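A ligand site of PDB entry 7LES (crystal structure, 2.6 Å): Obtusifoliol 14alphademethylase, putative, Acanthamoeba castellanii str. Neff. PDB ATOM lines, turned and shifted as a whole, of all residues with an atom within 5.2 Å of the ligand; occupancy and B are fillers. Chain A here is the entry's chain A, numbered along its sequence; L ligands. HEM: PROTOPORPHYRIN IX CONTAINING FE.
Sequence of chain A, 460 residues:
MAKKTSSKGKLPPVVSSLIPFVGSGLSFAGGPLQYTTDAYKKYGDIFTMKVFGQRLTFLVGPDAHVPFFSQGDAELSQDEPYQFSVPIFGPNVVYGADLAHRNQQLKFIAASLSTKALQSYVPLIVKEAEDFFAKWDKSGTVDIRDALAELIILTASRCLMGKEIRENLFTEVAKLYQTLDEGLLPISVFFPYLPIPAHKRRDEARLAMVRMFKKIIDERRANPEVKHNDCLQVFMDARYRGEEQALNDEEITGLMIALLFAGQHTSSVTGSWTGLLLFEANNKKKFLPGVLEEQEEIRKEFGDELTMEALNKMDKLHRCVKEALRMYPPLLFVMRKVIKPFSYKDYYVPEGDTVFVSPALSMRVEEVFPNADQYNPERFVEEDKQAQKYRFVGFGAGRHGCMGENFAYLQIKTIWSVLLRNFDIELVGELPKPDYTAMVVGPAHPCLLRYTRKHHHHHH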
ATOM      1  N   PHE A  68     -17.328  -1.202   1.918  1.00  0.00           N
ATOM      2  CA  PHE A  68     -17.179   0.021   2.711  1.00  0.00           C
ATOM      3  C   PHE A  68     -18.522   0.497   3.229  1.00  0.00           C
ATOM      4  O   PHE A  68     -18.680   0.708   4.443  1.00  0.00           O
ATOM      5  CB  PHE A  68     -16.506   1.117   1.866  1.00  0.00           C
ATOM      6  CG  PHE A  68     -16.038   2.287   2.668  1.00  0.00           C
ATOM      7  CD1 PHE A  68     -16.907   3.322   2.951  1.00  0.00           C
ATOM      8  CD2 PHE A  68     -14.742   2.334   3.138  1.00  0.00           C
ATOM      9  CE1 PHE A  68     -16.508   4.406   3.694  1.00  0.00           C
ATOM     10  CE2 PHE A  68     -14.325   3.425   3.893  1.00  0.00           C
ATOM     11  CZ  PHE A  68     -15.207   4.457   4.172  1.00  0.00           C
ATOM     12  N   PHE A  69     -19.481   0.675   2.328  1.00  0.00           N
ATOM     13  CA  PHE A  69     -20.763   1.258   2.714  1.00  0.00           C
ATOM     14  C   PHE A  69     -21.759   0.260   3.323  1.00  0.00           C
ATOM     15  O   PHE A  69     -22.546   0.632   4.217  1.00  0.00           O
ATOM     16  CB  PHE A  69     -21.322   2.078   1.547  1.00  0.00           C
ATOM     17  CG  PHE A  69     -20.451   3.275   1.198  1.00  0.00           C
ATOM     18  CD1 PHE A  69     -20.125   4.239   2.173  1.00  0.00           C
ATOM     19  CD2 PHE A  69     -19.929   3.443  -0.084  1.00  0.00           C
ATOM     20  CE1 PHE A  69     -19.316   5.328   1.857  1.00  0.00           C
ATOM     21  CE2 PHE A  69     -19.130   4.541  -0.398  1.00  0.00           C
ATOM     22  CZ  PHE A  69     -18.832   5.476   0.569  1.00  0.00           C
ATOM     23  N   GLN A  78     -14.926   4.203  12.868  1.00  0.00           N
ATOM     24  CA  GLN A  78     -14.689   5.603  12.566  1.00  0.00           C
ATOM     25  C   GLN A  78     -13.889   6.274  13.676  1.00  0.00           C
ATOM     26  O   GLN A  78     -13.561   7.438  13.547  1.00  0.00           O
ATOM     27  CB  GLN A  78     -16.013   6.373  12.427  1.00  0.00           C
ATOM     28  CG  GLN A  78     -16.942   5.934  11.317  1.00  0.00           C
ATOM     29  CD  GLN A  78     -18.122   6.877  11.167  1.00  0.00           C
ATOM     30  OE1 GLN A  78     -18.950   7.037  12.089  1.00  0.00           O
ATOM     31  NE2 GLN A  78     -18.198   7.527  10.013  1.00  0.00           N
ATOM     32  N   TYR A  82     -11.358   9.813  12.983  1.00  0.00           N
ATOM     33  CA  TYR A  82     -12.020  11.020  13.441  1.00  0.00           C
ATOM     34  C   TYR A  82     -11.564  11.386  14.872  1.00  0.00           C
ATOM     35  O   TYR A  82     -12.138  12.257  15.498  1.00  0.00           O
ATOM     36  CB  TYR A  82     -13.562  10.898  13.284  1.00  0.00           C
ATOM     37  CG  TYR A  82     -14.079  10.858  11.809  1.00  0.00           C
ATOM     38  CD1 TYR A  82     -13.825   9.762  10.973  1.00  0.00           C
ATOM     39  CD2 TYR A  82     -14.824  11.922  11.277  1.00  0.00           C
ATOM     40  CE1 TYR A  82     -14.294   9.741   9.661  1.00  0.00           C
ATOM     41  CE2 TYR A  82     -15.297  11.897   9.956  1.00  0.00           C
ATOM     42  CZ  TYR A  82     -15.026  10.809   9.168  1.00  0.00           C
ATOM     43  OH  TYR A  82     -15.493  10.785   7.880  1.00  0.00           O
ATOM     44  N   TYR A  95     -17.438  11.442  18.338  1.00  0.00           N
ATOM     45  CA  TYR A  95     -16.371  10.446  18.294  1.00  0.00           C
ATOM     46  C   TYR A  95     -15.617  10.498  19.599  1.00  0.00           C
ATOM     47  O   TYR A  95     -14.759   9.674  19.813  1.00  0.00           O
ATOM     48  CB  TYR A  95     -15.434  10.653  17.086  1.00  0.00           C
ATOM     49  CG  TYR A  95     -16.194  10.715  15.772  1.00  0.00           C
ATOM     50  CD1 TYR A  95     -16.745   9.572  15.204  1.00  0.00           C
ATOM     51  CD2 TYR A  95     -16.396  11.928  15.116  1.00  0.00           C
ATOM     52  CE1 TYR A  95     -17.472   9.620  14.025  1.00  0.00           C
ATOM     53  CE2 TYR A  95     -17.116  11.985  13.929  1.00  0.00           C
ATOM     54  CZ  TYR A  95     -17.654  10.830  13.384  1.00  0.00           C
ATOM     55  OH  TYR A  95     -18.381  10.878  12.205  1.00  0.00           O
ATOM     56  N   LEU A 106     -26.194  10.672  17.305  1.00  0.00           N
ATOM     57  CA  LEU A 106     -26.460  10.702  15.864  1.00  0.00           C
ATOM     58  C   LEU A 106     -27.948  10.687  15.542  1.00  0.00           C
ATOM     59  O   LEU A 106     -28.401  11.342  14.595  1.00  0.00           O
ATOM     60  CB  LEU A 106     -25.720   9.580  15.125  1.00  0.00           C
ATOM     61  CG  LEU A 106     -24.187   9.726  15.030  1.00  0.00           C
ATOM     62  CD1 LEU A 106     -23.569   8.434  14.498  1.00  0.00           C
ATOM     63  CD2 LEU A 106     -23.731  10.914  14.173  1.00  0.00           C
ATOM     64  N   ILE A 109     -29.255  14.380  16.214  1.00  0.00           N
ATOM     65  CA  ILE A 109     -28.818  15.106  15.025  1.00  0.00           C
ATOM     66  C   ILE A 109     -29.757  14.839  13.859  1.00  0.00           C
ATOM     67  O   ILE A 109     -30.138  15.763  13.174  1.00  0.00           O
ATOM     68  CB  ILE A 109     -27.342  14.735  14.655  1.00  0.00           C
ATOM     69  CG1 ILE A 109     -26.392  15.387  15.684  1.00  0.00           C
ATOM     70  CG2 ILE A 109     -26.998  15.164  13.227  1.00  0.00           C
ATOM     71  CD1 ILE A 109     -24.933  15.041  15.499  1.00  0.00           C
ATOM     72  N   LEU A 113     -32.380  17.355  11.593  1.00  0.00           N
ATOM     73  CA  LEU A 113     -32.341  17.476  10.119  1.00  0.00           C
ATOM     74  C   LEU A 113     -33.441  16.718   9.348  1.00  0.00           C
ATOM     75  O   LEU A 113     -33.365  16.603   8.115  1.00  0.00           O
ATOM     76  CB  LEU A 113     -30.966  17.011   9.615  1.00  0.00           C
ATOM     77  CG  LEU A 113     -29.736  17.714  10.173  1.00  0.00           C
ATOM     78  CD1 LEU A 113     -28.491  17.024   9.644  1.00  0.00           C
ATOM     79  CD2 LEU A 113     -29.740  19.183   9.797  1.00  0.00           C
ATOM     80  N   LEU A 160     -29.586  26.606  13.193  1.00  0.00           N
ATOM     81  CA  LEU A 160     -29.020  25.610  14.073  1.00  0.00           C
ATOM     82  C   LEU A 160     -28.975  26.151  15.495  1.00  0.00           C
ATOM     83  O   LEU A 160     -29.489  25.526  16.414  1.00  0.00           O
ATOM     84  CB  LEU A 160     -27.666  25.086  13.532  1.00  0.00           C
ATOM     85  CG  LEU A 160     -27.719  23.978  12.411  1.00  0.00           C
ATOM     86  CD1 LEU A 160     -28.885  24.085  11.413  1.00  0.00           C
ATOM     87  CD2 LEU A 160     -26.419  23.867  11.623  1.00  0.00           C
ATOM     88  N   LEU A 259     -22.117  20.216  13.979  1.00  0.00           N
ATOM     89  CA  LEU A 259     -22.945  20.611  12.845  1.00  0.00           C
ATOM     90  C   LEU A 259     -22.393  21.807  12.052  1.00  0.00           C
ATOM     91  O   LEU A 259     -22.503  21.859  10.819  1.00  0.00           O
ATOM     92  CB  LEU A 259     -24.374  20.899  13.297  1.00  0.00           C
ATOM     93  CG  LEU A 259     -25.223  19.691  13.663  1.00  0.00           C
ATOM     94  CD1 LEU A 259     -26.531  20.182  14.241  1.00  0.00           C
ATOM     95  CD2 LEU A 259     -25.514  18.781  12.471  1.00  0.00           C
ATOM     96  N   ALA A 262     -19.544  20.438   9.987  1.00  0.00           N
ATOM     97  CA  ALA A 262     -20.040  19.634   8.881  1.00  0.00           C
ATOM     98  C   ALA A 262     -20.609  20.556   7.837  1.00  0.00           C
ATOM     99  O   ALA A 262     -20.227  20.478   6.669  1.00  0.00           O
ATOM    100  CB  ALA A 262     -21.099  18.676   9.385  1.00  0.00           C
ATOM    101  N   GLY A 263     -21.497  21.453   8.264  1.00  0.00           N
ATOM    102  CA  GLY A 263     -22.231  22.322   7.352  1.00  0.00           C
ATOM    103  C   GLY A 263     -21.427  23.322   6.533  1.00  0.00           C
ATOM    104  O   GLY A 263     -21.586  23.380   5.314  1.00  0.00           O
ATOM    105  N   THR A 266     -18.172  22.513   3.443  1.00  0.00           N
ATOM    106  CA  THR A 266     -18.653  21.595   2.403  1.00  0.00           C
ATOM    107  C   THR A 266     -19.771  22.187   1.526  1.00  0.00           C
ATOM    108  O   THR A 266     -19.744  22.039   0.288  1.00  0.00           O
ATOM    109  CB  THR A 266     -19.125  20.281   3.015  1.00  0.00           C
ATOM    110  OG1 THR A 266     -20.037  20.564   4.070  1.00  0.00           O
ATOM    111  CG2 THR A 266     -17.940  19.544   3.569  1.00  0.00           C
ATOM    112  N   SER A 267     -20.739  22.861   2.172  1.00  0.00           N
ATOM    113  CA  SER A 267     -21.845  23.536   1.475  1.00  0.00           C
ATOM    114  C   SER A 267     -21.349  24.774   0.746  1.00  0.00           C
ATOM    115  O   SER A 267     -21.770  25.066  -0.384  1.00  0.00           O
ATOM    116  CB  SER A 267     -22.953  23.971   2.455  1.00  0.00           C
ATOM    117  OG  SER A 267     -23.345  22.949   3.364  1.00  0.00           O
ATOM    118  N   THR A 270     -19.213  23.712  -2.396  1.00  0.00           N
ATOM    119  CA  THR A 270     -20.091  23.088  -3.380  1.00  0.00           C
ATOM    120  C   THR A 270     -20.983  24.144  -4.046  1.00  0.00           C
ATOM    121  O   THR A 270     -21.071  24.200  -5.282  1.00  0.00           O
ATOM    122  CB  THR A 270     -20.920  21.977  -2.722  1.00  0.00           C
ATOM    123  OG1 THR A 270     -20.017  20.966  -2.255  1.00  0.00           O
ATOM    124  CG2 THR A 270     -21.937  21.370  -3.707  1.00  0.00           C
ATOM    125  N   LEU A 325     -20.771  18.618  -7.441  1.00  0.00           N
ATOM    126  CA  LEU A 325     -20.347  17.703  -6.388  1.00  0.00           C
ATOM    127  C   LEU A 325     -19.626  16.459  -6.902  1.00  0.00           C
ATOM    128  O   LEU A 325     -18.602  16.044  -6.344  1.00  0.00           O
ATOM    129  CB  LEU A 325     -21.583  17.307  -5.591  1.00  0.00           C
ATOM    130  CG  LEU A 325     -21.344  16.573  -4.298  1.00  0.00           C
ATOM    131  CD1 LEU A 325     -20.245  17.200  -3.469  1.00  0.00           C
ATOM    132  CD2 LEU A 325     -22.660  16.566  -3.537  1.00  0.00           C
ATOM    133  N   PRO A 330     -16.076  18.090  -1.954  1.00  0.00           N
ATOM    134  CA  PRO A 330     -15.308  18.758  -0.900  1.00  0.00           C
ATOM    135  C   PRO A 330     -14.511  17.834   0.000  1.00  0.00           C
ATOM    136  O   PRO A 330     -13.405  18.206   0.366  1.00  0.00           O
ATOM    137  CB  PRO A 330     -16.372  19.480  -0.082  1.00  0.00           C
ATOM    138  CG  PRO A 330     -17.625  18.765  -0.362  1.00  0.00           C
ATOM    139  CD  PRO A 330     -17.521  18.269  -1.767  1.00  0.00           C
ATOM    140  N   LEU A 331     -15.088  16.691   0.376  1.00  0.00           N
ATOM    141  CA  LEU A 331     -14.380  15.653   1.142  1.00  0.00           C
ATOM    142  C   LEU A 331     -13.821  14.601   0.195  1.00  0.00           C
ATOM    143  O   LEU A 331     -14.586  13.805  -0.361  1.00  0.00           O
ATOM    144  CB  LEU A 331     -15.328  14.951   2.113  1.00  0.00           C
ATOM    145  CG  LEU A 331     -16.027  15.780   3.178  1.00  0.00           C
ATOM    146  CD1 LEU A 331     -16.798  14.820   4.072  1.00  0.00           C
ATOM    147  CD2 LEU A 331     -15.044  16.627   3.967  1.00  0.00           C
ATOM    148  N   VAL A 334     -13.193   9.484   2.468  1.00  0.00           N
ATOM    149  CA  VAL A 334     -13.762   8.924   3.689  1.00  0.00           C
ATOM    150  C   VAL A 334     -13.064   7.623   4.043  1.00  0.00           C
ATOM    151  O   VAL A 334     -12.727   6.824   3.152  1.00  0.00           O
ATOM    152  CB  VAL A 334     -15.270   8.663   3.608  1.00  0.00           C
ATOM    153  CG1 VAL A 334     -16.005   9.974   3.507  1.00  0.00           C
ATOM    154  CG2 VAL A 334     -15.658   7.724   2.449  1.00  0.00           C
ATOM    155  N   MET A 335     -12.881   7.404   5.342  1.00  0.00           N
ATOM    156  CA  MET A 335     -12.110   6.285   5.821  1.00  0.00           C
ATOM    157  C   MET A 335     -12.662   5.578   7.071  1.00  0.00           C
ATOM    158  O   MET A 335     -13.342   6.173   7.929  1.00  0.00           O
ATOM    159  CB  MET A 335     -10.641   6.729   5.994  1.00  0.00           C
ATOM    160  CG  MET A 335     -10.316   7.546   7.243  1.00  0.00           C
ATOM    161  SD  MET A 335      -8.684   8.346   7.202  1.00  0.00           S
ATOM    162  CE  MET A 335      -9.065   9.806   6.222  1.00  0.00           C
ATOM    163  N   ARG A 336     -12.382   4.272   7.127  1.00  0.00           N
ATOM    164  CA  ARG A 336     -12.692   3.433   8.255  1.00  0.00           C
ATOM    165  C   ARG A 336     -11.460   2.561   8.592  1.00  0.00           C
ATOM    166  O   ARG A 336     -10.646   2.249   7.706  1.00  0.00           O
ATOM    167  CB  ARG A 336     -13.843   2.504   7.909  1.00  0.00           C
ATOM    168  CG  ARG A 336     -15.128   3.152   7.403  1.00  0.00           C
ATOM    169  CD  ARG A 336     -16.034   3.593   8.547  1.00  0.00           C
ATOM    170  NE  ARG A 336     -17.247   4.239   8.024  1.00  0.00           N
ATOM    171  CZ  ARG A 336     -17.310   5.489   7.567  1.00  0.00           C
ATOM    172  NH1 ARG A 336     -16.250   6.276   7.558  1.00  0.00           N
ATOM    173  NH2 ARG A 336     -18.460   5.955   7.111  1.00  0.00           N
ATOM    174  N   VAL A 393     -21.265   9.025  -4.806  1.00  0.00           N
ATOM    175  CA  VAL A 393     -20.843   8.902  -3.416  1.00  0.00           C
ATOM    176  C   VAL A 393     -20.265  10.205  -2.860  1.00  0.00           C
ATOM    177  O   VAL A 393     -19.398  10.180  -1.995  1.00  0.00           O
ATOM    178  CB  VAL A 393     -19.765   7.788  -3.303  1.00  0.00           C
ATOM    179  CG1 VAL A 393     -20.386   6.406  -3.478  1.00  0.00           C
ATOM    180  CG2 VAL A 393     -18.652   8.023  -4.330  1.00  0.00           C
ATOM    181  N   GLY A 394     -20.722  11.345  -3.359  1.00  0.00           N
ATOM    182  CA  GLY A 394     -20.333  12.633  -2.809  1.00  0.00           C
ATOM    183  C   GLY A 394     -20.740  12.780  -1.347  1.00  0.00           C
ATOM    184  O   GLY A 394     -20.041  13.472  -0.609  1.00  0.00           O
ATOM    185  N   PHE A 395     -21.832  12.115  -0.939  1.00  0.00           N
ATOM    186  CA  PHE A 395     -22.372  12.165   0.433  1.00  0.00           C
ATOM    187  C   PHE A 395     -22.214  10.837   1.189  1.00  0.00           C
ATOM    188  O   PHE A 395     -22.978  10.552   2.119  1.00  0.00           O
ATOM    189  CB  PHE A 395     -23.894  12.507   0.409  1.00  0.00           C
ATOM    190  CG  PHE A 395     -24.241  13.896  -0.078  1.00  0.00           C
ATOM    191  CD1 PHE A 395     -24.140  15.000   0.770  1.00  0.00           C
ATOM    192  CD2 PHE A 395     -24.742  14.090  -1.366  1.00  0.00           C
ATOM    193  CE1 PHE A 395     -24.470  16.273   0.312  1.00  0.00           C
ATOM    194  CE2 PHE A 395     -25.090  15.364  -1.814  1.00  0.00           C
ATOM    195  CZ  PHE A 395     -24.960  16.449  -0.975  1.00  0.00           C
ATOM    196  N   GLY A 396     -21.232  10.026   0.805  1.00  0.00           N
ATOM    197  CA  GLY A 396     -21.070   8.670   1.373  1.00  0.00           C
ATOM    198  C   GLY A 396     -22.300   7.811   1.129  1.00  0.00           C
ATOM    199  O   GLY A 396     -23.091   8.071   0.218  1.00  0.00           O
ATOM    200  N   ARG A 399     -24.821   3.099   6.731  1.00  0.00           N
ATOM    201  CA  ARG A 399     -25.000   3.445   8.146  1.00  0.00           C
ATOM    202  C   ARG A 399     -24.643   4.909   8.465  1.00  0.00           C
ATOM    203  O   ARG A 399     -25.414   5.577   9.110  1.00  0.00           O
ATOM    204  CB  ARG A 399     -24.201   2.456   9.011  1.00  0.00           C
ATOM    205  CG  ARG A 399     -24.202   2.736  10.511  1.00  0.00           C
ATOM    206  CD  ARG A 399     -25.568   2.534  11.127  1.00  0.00           C
ATOM    207  NE  ARG A 399     -26.004   3.685  11.910  1.00  0.00           N
ATOM    208  CZ  ARG A 399     -25.649   3.956  13.168  1.00  0.00           C
ATOM    209  NH1 ARG A 399     -24.818   3.164  13.830  1.00  0.00           N
ATOM    210  NH2 ARG A 399     -26.131   5.040  13.773  1.00  0.00           N
ATOM    211  N   HIS A 400     -23.497   5.385   7.970  1.00  0.00           N
ATOM    212  CA  HIS A 400     -22.994   6.749   8.260  1.00  0.00           C
ATOM    213  C   HIS A 400     -22.928   7.714   7.072  1.00  0.00           C
ATOM    214  O   HIS A 400     -22.092   8.624   7.078  1.00  0.00           O
ATOM    215  CB  HIS A 400     -21.615   6.644   8.871  1.00  0.00           C
ATOM    216  CG  HIS A 400     -21.618   5.956  10.186  1.00  0.00           C
ATOM    217  ND1 HIS A 400     -22.083   6.567  11.332  1.00  0.00           N
ATOM    218  CD2 HIS A 400     -21.243   4.712  10.543  1.00  0.00           C
ATOM    219  CE1 HIS A 400     -21.990   5.723  12.337  1.00  0.00           C
ATOM    220  NE2 HIS A 400     -21.484   4.587  11.890  1.00  0.00           N
ATOM    221  N   GLY A 401     -23.801   7.558   6.079  1.00  0.00           N
ATOM    222  CA  GLY A 401     -23.908   8.516   4.971  1.00  0.00           C
ATOM    223  C   GLY A 401     -24.444   9.850   5.486  1.00  0.00           C
ATOM    224  O   GLY A 401     -24.996   9.911   6.600  1.00  0.00           O
ATOM    225  N   CYS A 402     -24.275  10.908   4.692  1.00  0.00           N
ATOM    226  CA  CYS A 402     -24.652  12.278   5.123  1.00  0.00           C
ATOM    227  C   CYS A 402     -26.136  12.445   5.499  1.00  0.00           C
ATOM    228  O   CYS A 402     -27.029  12.293   4.628  1.00  0.00           O
ATOM    229  CB  CYS A 402     -24.285  13.338   4.052  1.00  0.00           C
ATOM    230  SG  CYS A 402     -24.407  15.091   4.563  1.00  0.00           S
ATOM    231  N   MET A 403     -26.373  12.743   6.796  1.00  0.00           N
ATOM    232  CA  MET A 403     -27.658  13.213   7.295  1.00  0.00           C
ATOM    233  C   MET A 403     -28.058  14.635   6.875  1.00  0.00           C
ATOM    234  O   MET A 403     -29.225  14.991   6.983  1.00  0.00           O
ATOM    235  CB  MET A 403     -27.686  13.160   8.807  1.00  0.00           C
ATOM    236  CG  MET A 403     -27.928  11.772   9.317  1.00  0.00           C
ATOM    237  SD  MET A 403     -27.914  11.890  11.101  1.00  0.00           S
ATOM    238  CE  MET A 403     -27.227  10.290  11.493  1.00  0.00           C
ATOM    239  N   GLY A 404     -27.092  15.428   6.410  1.00  0.00           N
ATOM    240  CA  GLY A 404     -27.359  16.769   5.923  1.00  0.00           C
ATOM    241  C   GLY A 404     -27.616  16.914   4.438  1.00  0.00           C
ATOM    242  O   GLY A 404     -27.855  18.044   3.977  1.00  0.00           O
ATOM    243  N   GLU A 405     -27.594  15.809   3.680  1.00  0.00           N
ATOM    244  CA  GLU A 405     -27.829  15.858   2.213  1.00  0.00           C
ATOM    245  C   GLU A 405     -28.948  16.822   1.793  1.00  0.00           C
ATOM    246  O   GLU A 405     -28.777  17.585   0.843  1.00  0.00           O
ATOM    247  CB  GLU A 405     -28.066  14.449   1.626  1.00  0.00           C
ATOM    248  CG  GLU A 405     -28.284  14.421   0.108  1.00  0.00           C
ATOM    249  CD  GLU A 405     -27.973  13.095  -0.612  1.00  0.00           C
ATOM    250  OE1 GLU A 405     -28.177  13.053  -1.848  1.00  0.00           O
ATOM    251  OE2 GLU A 405     -27.505  12.108   0.024  1.00  0.00           O
ATOM    252  N   PHE A 407     -30.675  19.449   3.682  1.00  0.00           N
ATOM    253  CA  PHE A 407     -30.346  20.807   4.089  1.00  0.00           C
ATOM    254  C   PHE A 407     -29.353  21.397   3.077  1.00  0.00           C
ATOM    255  O   PHE A 407     -29.481  22.544   2.667  1.00  0.00           O
ATOM    256  CB  PHE A 407     -29.778  20.824   5.531  1.00  0.00           C
ATOM    257  CG  PHE A 407     -29.294  22.181   6.007  1.00  0.00           C
ATOM    258  CD1 PHE A 407     -28.037  22.682   5.622  1.00  0.00           C
ATOM    259  CD2 PHE A 407     -30.056  22.926   6.885  1.00  0.00           C
ATOM    260  CE1 PHE A 407     -27.563  23.902   6.078  1.00  0.00           C
ATOM    261  CE2 PHE A 407     -29.593  24.156   7.342  1.00  0.00           C
ATOM    262  CZ  PHE A 407     -28.357  24.637   6.941  1.00  0.00           C
ATOM    263  N   ALA A 408     -28.364  20.611   2.666  1.00  0.00           N
ATOM    264  CA  ALA A 408     -27.330  21.126   1.762  1.00  0.00           C
ATOM    265  C   ALA A 408     -27.898  21.536   0.420  1.00  0.00           C
ATOM    266  O   ALA A 408     -27.607  22.624  -0.087  1.00  0.00           O
ATOM    267  CB  ALA A 408     -26.236  20.098   1.567  1.00  0.00           C
ATOM    268  N   ILE A 412     -28.163  25.388  -1.023  1.00  0.00           N
ATOM    269  CA  ILE A 412     -27.509  25.740  -2.277  1.00  0.00           C
ATOM    270  C   ILE A 412     -28.525  26.101  -3.336  1.00  0.00           C
ATOM    271  O   ILE A 412     -28.304  27.035  -4.081  1.00  0.00           O
ATOM    272  CB  ILE A 412     -26.560  24.640  -2.739  1.00  0.00           C
ATOM    273  CG1 ILE A 412     -25.400  24.561  -1.751  1.00  0.00           C
ATOM    274  CG2 ILE A 412     -26.021  24.925  -4.132  1.00  0.00           C
ATOM    275  CD1 ILE A 412     -24.458  23.414  -2.028  1.00  0.00           C
HETATM  276  CHA HEM L   1     -21.567  12.520   6.862  1.00  0.00           C
HETATM  277  CHB HEM L   1     -20.565  14.925   2.792  1.00  0.00           C
HETATM  278  CHC HEM L   1     -23.329  18.622   4.242  1.00  0.00           C
HETATM  279  CHD HEM L   1     -23.877  16.452   8.475  1.00  0.00           C
HETATM  280  C1A HEM L   1     -21.080  12.843   5.619  1.00  0.00           C
HETATM  281  C2A HEM L   1     -20.242  12.006   4.811  1.00  0.00           C
HETATM  282  C3A HEM L   1     -19.951  12.699   3.671  1.00  0.00           C
HETATM  283  C4A HEM L   1     -20.605  13.961   3.766  1.00  0.00           C
HETATM  284  CMA HEM L   1     -19.125  12.230   2.487  1.00  0.00           C
HETATM  285  CAA HEM L   1     -19.768  10.612   5.138  1.00  0.00           C
HETATM  286  CBA HEM L   1     -18.596  10.614   6.109  1.00  0.00           C
HETATM  287  CGA HEM L   1     -18.179   9.209   6.437  1.00  0.00           C
HETATM  288  O1A HEM L   1     -18.701   8.204   5.880  1.00  0.00           O
HETATM  289  O2A HEM L   1     -17.296   9.022   7.289  1.00  0.00           O
HETATM  290  C1B HEM L   1     -21.271  16.140   2.839  1.00  0.00           C
HETATM  291  C2B HEM L   1     -21.271  17.079   1.776  1.00  0.00           C
HETATM  292  C3B HEM L   1     -22.053  18.145   2.167  1.00  0.00           C
HETATM  293  C4B HEM L   1     -22.515  17.784   3.511  1.00  0.00           C
HETATM  294  CMB HEM L   1     -20.529  16.919   0.470  1.00  0.00           C
HETATM  295  CAB HEM L   1     -22.438  19.391   1.456  1.00  0.00           C
HETATM  296  CBB HEM L   1     -22.222  19.647   0.166  1.00  0.00           C
HETATM  297  C1C HEM L   1     -23.716  18.388   5.536  1.00  0.00           C
HETATM  298  C2C HEM L   1     -24.394  19.329   6.342  1.00  0.00           C
HETATM  299  C3C HEM L   1     -24.561  18.718   7.596  1.00  0.00           C
HETATM  300  C4C HEM L   1     -23.962  17.398   7.484  1.00  0.00           C
HETATM  301  CMC HEM L   1     -24.870  20.695   5.892  1.00  0.00           C
HETATM  302  CAC HEM L   1     -25.206  19.227   8.830  1.00  0.00           C
HETATM  303  CBC HEM L   1     -25.732  20.428   9.025  1.00  0.00           C
HETATM  304  C1D HEM L   1     -23.285  15.200   8.313  1.00  0.00           C
HETATM  305  C2D HEM L   1     -23.304  14.240   9.422  1.00  0.00           C
HETATM  306  C3D HEM L   1     -22.705  13.137   8.956  1.00  0.00           C
HETATM  307  C4D HEM L   1     -22.276  13.442   7.594  1.00  0.00           C
HETATM  308  CMD HEM L   1     -23.908  14.409  10.804  1.00  0.00           C
HETATM  309  CAD HEM L   1     -22.399  11.908   9.768  1.00  0.00           C
HETATM  310  CBD HEM L   1     -23.137  10.623   9.533  1.00  0.00           C
HETATM  311  CGD HEM L   1     -22.642   9.659  10.590  1.00  0.00           C
HETATM  312  O1D HEM L   1     -21.481   9.649  11.126  1.00  0.00           O
HETATM  313  O2D HEM L   1     -23.502   8.817  10.939  1.00  0.00           O
HETATM  314  NA  HEM L   1     -21.263  14.054   4.978  1.00  0.00           N
HETATM  315  NB  HEM L   1     -22.003  16.595   3.826  1.00  0.00           N
HETATM  316  NC  HEM L   1     -23.441  17.257   6.238  1.00  0.00           N
HETATM  317  ND  HEM L   1     -22.653  14.696   7.234  1.00  0.00           N
HETATM  318 FE   HEM L   1     -22.328  15.599   5.599  1.00  0.00          FE
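The side-chain sulfur (SG) of Cys 402 is bound to an iron atom (FE) of the ligand (2.4 Å). NH2 of Arg 336 is in salt-bridge range of O1A of the ligand, 2.6 Å away. The side-chain hydroxyl of Tyr 82 sits at hydrogen-bond distance from an oxygen (O2A) of the ligand (2.6 Å). ND1 of His 400 lies within hydrogen-bond range of O2D of the ligand. NE2 of Gln 78 lies within hydrogen-bond range of O2A of the ligand (3.2 Å).
Residues that only touch the ligand: Tyr 95, Leu 106, Ile 109, Leu 259, Ala 262, Gly 263, Thr 266, Ser 267, Thr 270, Leu 325, Pro 330, Leu 331, Val 334, Gly 394, Phe 395, Gly 396, Gly 401, Gly 404, Phe 407 and Ala 408. Of the 35 residues printed, 25 come within 4 Å of the ligand.
O of Phe 395 lies within hydrogen-bond range of N of Cys 402, at 2.9 Å. SG of Cys 402 lies close to N of Gly 404 (3.3 Å). The backbone NH of Glu 405 sits close to the side-chain sulfur of Cys 402 (3.4 Å). The side-chain amide nitrogen (NE2) of Gln 78 sits close to the guanidinium group (NH2) of Arg 336, at 3.3 Å. O of Gly 263 is in hydrogen-bond range of OG1 of Thr 266 (3.4 Å). OG of Ser 267 is in hydrogen-bond range of O of Gly 263 (2.7 Å). OG1 of Thr 270 lies within hydrogen-bond range of O of Thr 266 (2.8 Å). The backbone carbonyl oxygen (O) of Ala 262 lies within hydrogen-bond range of the side-chain hydroxyl (OG1) of Thr 266, at 2.6 Å.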
